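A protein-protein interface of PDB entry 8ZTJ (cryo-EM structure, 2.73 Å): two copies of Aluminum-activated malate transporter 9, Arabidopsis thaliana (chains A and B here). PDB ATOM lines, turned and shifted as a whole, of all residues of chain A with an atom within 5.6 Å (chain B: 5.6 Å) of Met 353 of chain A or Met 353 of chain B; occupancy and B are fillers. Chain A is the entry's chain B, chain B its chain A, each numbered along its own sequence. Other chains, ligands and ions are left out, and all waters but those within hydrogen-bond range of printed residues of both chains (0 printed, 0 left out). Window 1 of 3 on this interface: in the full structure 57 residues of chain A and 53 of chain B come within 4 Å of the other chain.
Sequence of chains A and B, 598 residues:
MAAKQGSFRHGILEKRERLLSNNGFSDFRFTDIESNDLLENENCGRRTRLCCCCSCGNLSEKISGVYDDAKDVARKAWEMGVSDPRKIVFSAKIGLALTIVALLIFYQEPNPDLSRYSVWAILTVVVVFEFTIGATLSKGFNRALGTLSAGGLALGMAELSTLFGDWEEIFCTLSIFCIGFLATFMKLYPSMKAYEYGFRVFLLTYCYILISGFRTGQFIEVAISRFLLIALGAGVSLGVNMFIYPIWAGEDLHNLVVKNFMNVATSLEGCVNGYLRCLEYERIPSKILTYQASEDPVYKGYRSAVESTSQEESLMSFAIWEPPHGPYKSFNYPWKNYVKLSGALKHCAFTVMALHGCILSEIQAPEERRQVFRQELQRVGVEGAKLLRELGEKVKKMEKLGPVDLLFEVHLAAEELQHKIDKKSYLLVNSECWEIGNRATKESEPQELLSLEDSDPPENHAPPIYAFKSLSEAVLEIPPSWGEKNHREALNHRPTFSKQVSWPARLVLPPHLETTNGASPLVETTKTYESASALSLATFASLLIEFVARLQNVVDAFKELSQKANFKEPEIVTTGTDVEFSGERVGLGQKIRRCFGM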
ATOM      1  N   TYR A 302       3.978  -0.304 -25.392  1.00  0.00           N
ATOM      2  CA  TYR A 302       3.826  -1.297 -24.335  1.00  0.00           C
ATOM      3  C   TYR A 302       3.281  -2.617 -24.867  1.00  0.00           C
ATOM      4  O   TYR A 302       3.573  -3.675 -24.295  1.00  0.00           O
ATOM      5  CB  TYR A 302       2.951  -0.738 -23.207  1.00  0.00           C
ATOM      6  CG  TYR A 302       1.457  -0.731 -23.461  1.00  0.00           C
ATOM      7  CD1 TYR A 302       0.704  -1.894 -23.358  1.00  0.00           C
ATOM      8  CD2 TYR A 302       0.797   0.447 -23.781  1.00  0.00           C
ATOM      9  CE1 TYR A 302      -0.660  -1.884 -23.583  1.00  0.00           C
ATOM     10  CE2 TYR A 302      -0.565   0.466 -24.006  1.00  0.00           C
ATOM     11  CZ  TYR A 302      -1.288  -0.701 -23.907  1.00  0.00           C
ATOM     12  OH  TYR A 302      -2.645  -0.684 -24.128  1.00  0.00           O
ATOM     13  N   ARG A 303       2.525  -2.597 -25.970  1.00  0.00           N
ATOM     14  CA  ARG A 303       2.078  -3.860 -26.548  1.00  0.00           C
ATOM     15  C   ARG A 303       3.263  -4.714 -26.981  1.00  0.00           C
ATOM     16  O   ARG A 303       3.295  -5.923 -26.724  1.00  0.00           O
ATOM     17  CB  ARG A 303       1.144  -3.597 -27.729  1.00  0.00           C
ATOM     18  CG  ARG A 303      -0.279  -3.271 -27.323  1.00  0.00           C
ATOM     19  CD  ARG A 303      -0.868  -4.366 -26.449  1.00  0.00           C
ATOM     20  NE  ARG A 303      -2.168  -3.989 -25.907  1.00  0.00           N
ATOM     21  CZ  ARG A 303      -2.886  -4.744 -25.086  1.00  0.00           C
ATOM     22  NH1 ARG A 303      -2.471  -5.941 -24.709  1.00  0.00           N
ATOM     23  NH2 ARG A 303      -4.052  -4.288 -24.641  1.00  0.00           N
ATOM     24  N   VAL A 306       5.381  -5.960 -24.014  1.00  0.00           N
ATOM     25  CA  VAL A 306       4.747  -6.966 -23.166  1.00  0.00           C
ATOM     26  C   VAL A 306       4.424  -8.255 -23.908  1.00  0.00           C
ATOM     27  O   VAL A 306       4.036  -9.242 -23.259  1.00  0.00           O
ATOM     28  CB  VAL A 306       3.471  -6.414 -22.494  1.00  0.00           C
ATOM     29  CG1 VAL A 306       2.914  -7.414 -21.493  1.00  0.00           C
ATOM     30  CG2 VAL A 306       3.762  -5.087 -21.812  1.00  0.00           C
ATOM     31  N   ALA A 349       6.415  -1.794 -17.656  1.00  0.00           N
ATOM     32  CA  ALA A 349       5.457  -1.500 -18.717  1.00  0.00           C
ATOM     33  C   ALA A 349       4.029  -1.866 -18.329  1.00  0.00           C
ATOM     34  O   ALA A 349       3.077  -1.305 -18.891  1.00  0.00           O
ATOM     35  CB  ALA A 349       5.852  -2.229 -20.000  1.00  0.00           C
ATOM     36  N   PHE A 350       3.856  -2.807 -17.397  1.00  0.00           N
ATOM     37  CA  PHE A 350       2.497  -3.149 -16.968  1.00  0.00           C
ATOM     38  C   PHE A 350       1.746  -1.931 -16.425  1.00  0.00           C
ATOM     39  O   PHE A 350       0.571  -1.714 -16.755  1.00  0.00           O
ATOM     40  CB  PHE A 350       2.534  -4.261 -15.920  1.00  0.00           C
ATOM     41  CG  PHE A 350       2.681  -5.637 -16.501  1.00  0.00           C
ATOM     42  CD1 PHE A 350       1.905  -6.033 -17.578  1.00  0.00           C
ATOM     43  CD2 PHE A 350       3.586  -6.538 -15.967  1.00  0.00           C
ATOM     44  CE1 PHE A 350       2.034  -7.299 -18.115  1.00  0.00           C
ATOM     45  CE2 PHE A 350       3.720  -7.805 -16.501  1.00  0.00           C
ATOM     46  CZ  PHE A 350       2.942  -8.185 -17.576  1.00  0.00           C
ATOM     47  N   THR A 351       2.398  -1.124 -15.582  1.00  0.00           N
ATOM     48  CA  THR A 351       1.701   0.025 -15.012  1.00  0.00           C
ATOM     49  C   THR A 351       1.418   1.090 -16.066  1.00  0.00           C
ATOM     50  O   THR A 351       0.424   1.815 -15.959  1.00  0.00           O
ATOM     51  CB  THR A 351       2.498   0.619 -13.847  1.00  0.00           C
ATOM     52  OG1 THR A 351       1.982   1.916 -13.523  1.00  0.00           O
ATOM     53  CG2 THR A 351       3.963   0.743 -14.205  1.00  0.00           C
ATOM     54  N   VAL A 352       2.263   1.194 -17.093  1.00  0.00           N
ATOM     55  CA  VAL A 352       1.966   2.101 -18.197  1.00  0.00           C
ATOM     56  C   VAL A 352       0.732   1.624 -18.951  1.00  0.00           C
ATOM     57  O   VAL A 352      -0.101   2.428 -19.388  1.00  0.00           O
ATOM     58  CB  VAL A 352       3.184   2.235 -19.127  1.00  0.00           C
ATOM     59  CG1 VAL A 352       2.904   3.248 -20.224  1.00  0.00           C
ATOM     60  CG2 VAL A 352       4.417   2.630 -18.332  1.00  0.00           C
ATOM     61  N   MET A 353       0.599   0.307 -19.122  1.00  0.00           N
ATOM     62  CA  MET A 353      -0.617  -0.233 -19.723  1.00  0.00           C
ATOM     63  C   MET A 353      -1.845   0.116 -18.890  1.00  0.00           C
ATOM     64  O   MET A 353      -2.893   0.481 -19.434  1.00  0.00           O
ATOM     65  CB  MET A 353      -0.492  -1.747 -19.882  1.00  0.00           C
ATOM     66  CG  MET A 353      -1.790  -2.442 -20.255  1.00  0.00           C
ATOM     67  SD  MET A 353      -1.550  -4.173 -20.690  1.00  0.00           S
ATOM     68  CE  MET A 353      -3.242  -4.756 -20.703  1.00  0.00           C
ATOM     69  N   ALA A 354      -1.734   0.011 -17.566  1.00  0.00           N
ATOM     70  CA  ALA A 354      -2.851   0.393 -16.700  1.00  0.00           C
ATOM     71  C   ALA A 354      -3.179   1.881 -16.820  1.00  0.00           C
ATOM     72  O   ALA A 354      -4.356   2.272 -16.829  1.00  0.00           O
ATOM     73  CB  ALA A 354      -2.540   0.029 -15.250  1.00  0.00           C
ATOM     74  N   LEU A 355      -2.152   2.728 -16.906  1.00  0.00           N
ATOM     75  CA  LEU A 355      -2.384   4.158 -17.094  1.00  0.00           C
ATOM     76  C   LEU A 355      -3.094   4.441 -18.413  1.00  0.00           C
ATOM     77  O   LEU A 355      -3.990   5.292 -18.473  1.00  0.00           O
ATOM     78  CB  LEU A 355      -1.060   4.918 -17.025  1.00  0.00           C
ATOM     79  CG  LEU A 355      -0.516   5.239 -15.631  1.00  0.00           C
ATOM     80  CD1 LEU A 355       0.980   5.503 -15.684  1.00  0.00           C
ATOM     81  CD2 LEU A 355      -1.247   6.427 -15.032  1.00  0.00           C
ATOM     82  N   HIS A 356      -2.708   3.743 -19.483  1.00  0.00           N
ATOM     83  CA  HIS A 356      -3.445   3.875 -20.737  1.00  0.00           C
ATOM     84  C   HIS A 356      -4.886   3.407 -20.582  1.00  0.00           C
ATOM     85  O   HIS A 356      -5.808   4.011 -21.143  1.00  0.00           O
ATOM     86  CB  HIS A 356      -2.753   3.090 -21.850  1.00  0.00           C
ATOM     87  CG  HIS A 356      -3.522   3.067 -23.134  1.00  0.00           C
ATOM     88  ND1 HIS A 356      -3.797   1.903 -23.819  1.00  0.00           N
ATOM     89  CD2 HIS A 356      -4.085   4.067 -23.853  1.00  0.00           C
ATOM     90  CE1 HIS A 356      -4.491   2.188 -24.906  1.00  0.00           C
ATOM     91  NE2 HIS A 356      -4.678   3.494 -24.951  1.00  0.00           N
ATOM     92  N   GLY A 357      -5.100   2.330 -19.827  1.00  0.00           N
ATOM     93  CA  GLY A 357      -6.454   1.853 -19.602  1.00  0.00           C
ATOM     94  C   GLY A 357      -7.322   2.867 -18.886  1.00  0.00           C
ATOM     95  O   GLY A 357      -8.527   2.951 -19.140  1.00  0.00           O
ATOM     96  N   CYS A 358      -6.728   3.647 -17.982  1.00  0.00           N
ATOM     97  CA  CYS A 358      -7.489   4.671 -17.269  1.00  0.00           C
ATOM     98  C   CYS A 358      -8.120   5.698 -18.204  1.00  0.00           C
ATOM     99  O   CYS A 358      -9.104   6.341 -17.822  1.00  0.00           O
ATOM    100  CB  CYS A 358      -6.601   5.390 -16.251  1.00  0.00           C
ATOM    101  SG  CYS A 358      -5.718   4.307 -15.110  1.00  0.00           S
ATOM    102  N   TYR B 302      -7.404 -14.815 -16.103  1.00  0.00           N
ATOM    103  CA  TYR B 302      -7.363 -13.635 -16.958  1.00  0.00           C
ATOM    104  C   TYR B 302      -6.257 -13.728 -18.002  1.00  0.00           C
ATOM    105  O   TYR B 302      -6.392 -13.154 -19.089  1.00  0.00           O
ATOM    106  CB  TYR B 302      -7.221 -12.372 -16.099  1.00  0.00           C
ATOM    107  CG  TYR B 302      -5.832 -12.092 -15.563  1.00  0.00           C
ATOM    108  CD1 TYR B 302      -4.844 -11.543 -16.370  1.00  0.00           C
ATOM    109  CD2 TYR B 302      -5.516 -12.362 -14.237  1.00  0.00           C
ATOM    110  CE1 TYR B 302      -3.580 -11.284 -15.876  1.00  0.00           C
ATOM    111  CE2 TYR B 302      -4.256 -12.105 -13.736  1.00  0.00           C
ATOM    112  CZ  TYR B 302      -3.293 -11.566 -14.558  1.00  0.00           C
ATOM    113  OH  TYR B 302      -2.036 -11.308 -14.063  1.00  0.00           O
ATOM    114  N   ARG B 303      -5.178 -14.465 -17.723  1.00  0.00           N
ATOM    115  CA  ARG B 303      -4.157 -14.644 -18.751  1.00  0.00           C
ATOM    116  C   ARG B 303      -4.713 -15.388 -19.958  1.00  0.00           C
ATOM    117  O   ARG B 303      -4.456 -15.005 -21.105  1.00  0.00           O
ATOM    118  CB  ARG B 303      -2.948 -15.376 -18.174  1.00  0.00           C
ATOM    119  CG  ARG B 303      -2.021 -14.471 -17.394  1.00  0.00           C
ATOM    120  CD  ARG B 303      -1.601 -13.276 -18.235  1.00  0.00           C
ATOM    121  NE  ARG B 303      -0.852 -12.295 -17.462  1.00  0.00           N
ATOM    122  CZ  ARG B 303      -0.425 -11.134 -17.940  1.00  0.00           C
ATOM    123  NH1 ARG B 303      -0.652 -10.777 -19.193  1.00  0.00           N
ATOM    124  NH2 ARG B 303       0.248 -10.311 -17.140  1.00  0.00           N
ATOM    125  N   VAL B 306      -7.160 -13.249 -21.911  1.00  0.00           N
ATOM    126  CA  VAL B 306      -6.575 -12.117 -22.623  1.00  0.00           C
ATOM    127  C   VAL B 306      -5.545 -12.540 -23.658  1.00  0.00           C
ATOM    128  O   VAL B 306      -5.033 -11.680 -24.390  1.00  0.00           O
ATOM    129  CB  VAL B 306      -5.957 -11.101 -21.640  1.00  0.00           C
ATOM    130  CG1 VAL B 306      -5.503  -9.851 -22.375  1.00  0.00           C
ATOM    131  CG2 VAL B 306      -6.955 -10.744 -20.550  1.00  0.00           C
ATOM    132  N   ALA B 349     -11.857  -8.350 -18.586  1.00  0.00           N
ATOM    133  CA  ALA B 349     -10.731  -9.029 -17.949  1.00  0.00           C
ATOM    134  C   ALA B 349      -9.544  -8.095 -17.738  1.00  0.00           C
ATOM    135  O   ALA B 349      -8.717  -8.330 -16.844  1.00  0.00           O
ATOM    136  CB  ALA B 349     -10.309 -10.241 -18.777  1.00  0.00           C
ATOM    137  N   PHE B 350      -9.421  -7.054 -18.564  1.00  0.00           N
ATOM    138  CA  PHE B 350      -8.321  -6.109 -18.362  1.00  0.00           C
ATOM    139  C   PHE B 350      -8.365  -5.484 -16.966  1.00  0.00           C
ATOM    140  O   PHE B 350      -7.322  -5.309 -16.315  1.00  0.00           O
ATOM    141  CB  PHE B 350      -8.347  -5.020 -19.434  1.00  0.00           C
ATOM    142  CG  PHE B 350      -7.770  -5.451 -20.752  1.00  0.00           C
ATOM    143  CD1 PHE B 350      -6.572  -6.144 -20.804  1.00  0.00           C
ATOM    144  CD2 PHE B 350      -8.417  -5.152 -21.939  1.00  0.00           C
ATOM    145  CE1 PHE B 350      -6.035  -6.540 -22.014  1.00  0.00           C
ATOM    146  CE2 PHE B 350      -7.884  -5.545 -23.151  1.00  0.00           C
ATOM    147  CZ  PHE B 350      -6.692  -6.240 -23.189  1.00  0.00           C
ATOM    148  N   THR B 351      -9.562  -5.142 -16.483  1.00  0.00           N
ATOM    149  CA  THR B 351      -9.676  -4.547 -15.155  1.00  0.00           C
ATOM    150  C   THR B 351      -9.274  -5.536 -14.068  1.00  0.00           C
ATOM    151  O   THR B 351      -8.680  -5.148 -13.056  1.00  0.00           O
ATOM    152  CB  THR B 351     -11.100  -4.044 -14.925  1.00  0.00           C
ATOM    153  OG1 THR B 351     -11.508  -3.235 -16.034  1.00  0.00           O
ATOM    154  CG2 THR B 351     -11.171  -3.214 -13.656  1.00  0.00           C
ATOM    155  N   VAL B 352      -9.595  -6.817 -14.251  1.00  0.00           N
ATOM    156  CA  VAL B 352      -9.183  -7.824 -13.278  1.00  0.00           C
ATOM    157  C   VAL B 352      -7.667  -7.961 -13.271  1.00  0.00           C
ATOM    158  O   VAL B 352      -7.050  -8.173 -12.220  1.00  0.00           O
ATOM    159  CB  VAL B 352      -9.877  -9.166 -13.569  1.00  0.00           C
ATOM    160  CG1 VAL B 352      -9.486 -10.200 -12.524  1.00  0.00           C
ATOM    161  CG2 VAL B 352     -11.388  -8.986 -13.614  1.00  0.00           C
ATOM    162  N   MET B 353      -7.042  -7.850 -14.443  1.00  0.00           N
ATOM    163  CA  MET B 353      -5.583  -7.861 -14.490  1.00  0.00           C
ATOM    164  C   MET B 353      -4.997  -6.678 -13.722  1.00  0.00           C
ATOM    165  O   MET B 353      -4.012  -6.826 -12.987  1.00  0.00           O
ATOM    166  CB  MET B 353      -5.101  -7.844 -15.940  1.00  0.00           C
ATOM    167  CG  MET B 353      -3.598  -7.731 -16.078  1.00  0.00           C
ATOM    168  SD  MET B 353      -3.087  -7.106 -17.689  1.00  0.00           S
ATOM    169  CE  MET B 353      -3.566  -8.461 -18.752  1.00  0.00           C
ATOM    170  N   ALA B 354      -5.595  -5.493 -13.874  1.00  0.00           N
ATOM    171  CA  ALA B 354      -5.137  -4.341 -13.097  1.00  0.00           C
ATOM    172  C   ALA B 354      -5.326  -4.560 -11.595  1.00  0.00           C
ATOM    173  O   ALA B 354      -4.458  -4.202 -10.786  1.00  0.00           O
ATOM    174  CB  ALA B 354      -5.868  -3.077 -13.551  1.00  0.00           C
ATOM    175  N   LEU B 355      -6.453  -5.155 -11.203  1.00  0.00           N
ATOM    176  CA  LEU B 355      -6.681  -5.435  -9.788  1.00  0.00           C
ATOM    177  C   LEU B 355      -5.647  -6.412  -9.242  1.00  0.00           C
ATOM    178  O   LEU B 355      -5.174  -6.258  -8.110  1.00  0.00           O
ATOM    179  CB  LEU B 355      -8.094  -5.978  -9.576  1.00  0.00           C
ATOM    180  CG  LEU B 355      -9.222  -4.946  -9.535  1.00  0.00           C
ATOM    181  CD1 LEU B 355     -10.568  -5.609  -9.783  1.00  0.00           C
ATOM    182  CD2 LEU B 355      -9.218  -4.209  -8.207  1.00  0.00           C
ATOM    183  N   HIS B 356      -5.284  -7.428 -10.027  1.00  0.00           N
ATOM    184  CA  HIS B 356      -4.219  -8.330  -9.600  1.00  0.00           C
ATOM    185  C   HIS B 356      -2.893  -7.592  -9.467  1.00  0.00           C
ATOM    186  O   HIS B 356      -2.143  -7.814  -8.511  1.00  0.00           O
ATOM    187  CB  HIS B 356      -4.079  -9.496 -10.575  1.00  0.00           C
ATOM    188  CG  HIS B 356      -3.019 -10.477 -10.186  1.00  0.00           C
ATOM    189  ND1 HIS B 356      -2.160 -11.049 -11.100  1.00  0.00           N
ATOM    190  CD2 HIS B 356      -2.673 -10.982  -8.978  1.00  0.00           C
ATOM    191  CE1 HIS B 356      -1.333 -11.865 -10.472  1.00  0.00           C
ATOM    192  NE2 HIS B 356      -1.623 -11.844  -9.185  1.00  0.00           N
ATOM    193  N   GLY B 357      -2.588  -6.710 -10.420  1.00  0.00           N
ATOM    194  CA  GLY B 357      -1.378  -5.912 -10.308  1.00  0.00           C
ATOM    195  C   GLY B 357      -1.353  -5.053  -9.060  1.00  0.00           C
ATOM    196  O   GLY B 357      -0.281  -4.752  -8.528  1.00  0.00           O
ATOM    197  N   CYS B 358      -2.529  -4.643  -8.581  1.00  0.00           N
ATOM    198  CA  CYS B 358      -2.599  -3.854  -7.353  1.00  0.00           C
ATOM    199  C   CYS B 358      -1.987  -4.582  -6.158  1.00  0.00           C
ATOM    200  O   CYS B 358      -1.432  -3.937  -5.262  1.00  0.00           O
ATOM    201  CB  CYS B 358      -4.051  -3.483  -7.049  1.00  0.00           C
ATOM    202  SG  CYS B 358      -4.523  -1.807  -7.534  1.00  0.00           S
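Among the printed residues, merely in contact across the chains: Phe 350 of chain A with Arg 303 of chain B (3.5 Å), Met 353 of chain A with Phe 350 of chain B (3.6 Å), Arg 303 of chain A with Phe 350 of chain B (3.6 Å) and Met 353 of chain A with Met 353 of chain B (3.8 Å).
Printed residues of chain B that touch a printed residue of chain A: Arg 303, Phe 350 and Met 353.
Hydrophobic or aromatic side chains of chain B that line the printed part of chain A: Phe 350 and Met 353.
Of the 13 printed residues of chain A, 3 touch a printed residue of chain B.
Among the printed residues, no Asp or Glu carboxylate lies within 4 Å of a Lys or Arg side-chain nitrogen of the other chain.
Arg 303 of chain A touches Phe 350 of chain B, and with the chains exchanged Phe 350 of chain A touches Arg 303 of chain B.
Met 353 of chain A touches Phe 350 of chain B, but with the chains exchanged Phe 350 of chain A does not touch Met 353 of chain B (5.1 Å).
Met 353 of chain B touches its own counterpart, Met 353 of chain A.
13 positions are printed for both chains.
Of the 4 pairs that touch across the chains among the printed residues, 3 have their exchanged pair printed and touching as well.
Of the printed residues of chain B, Met 353 of chain A touches Phe 350 and Met 353.
Met 353 of chain B touches one residue of chain A.
Of the printed residues of chain A, Arg 303 of chain B touches Phe 350.
Printed residues of chain A within 4 Å of Phe 350 of chain B: Arg 303 and Met 353.
Of the printed residues of chain B, Arg 303 of chain A touches Phe 350 (3.6 Å).
Of the printed residues of chain B, Phe 350 of chain A touches Arg 303.
Val 352 of chain A touches none of the printed residues of chain B.
The nearest residue of chain A that does not touch Met 353 of chain B is Phe 350 of chain A (5.1 Å).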
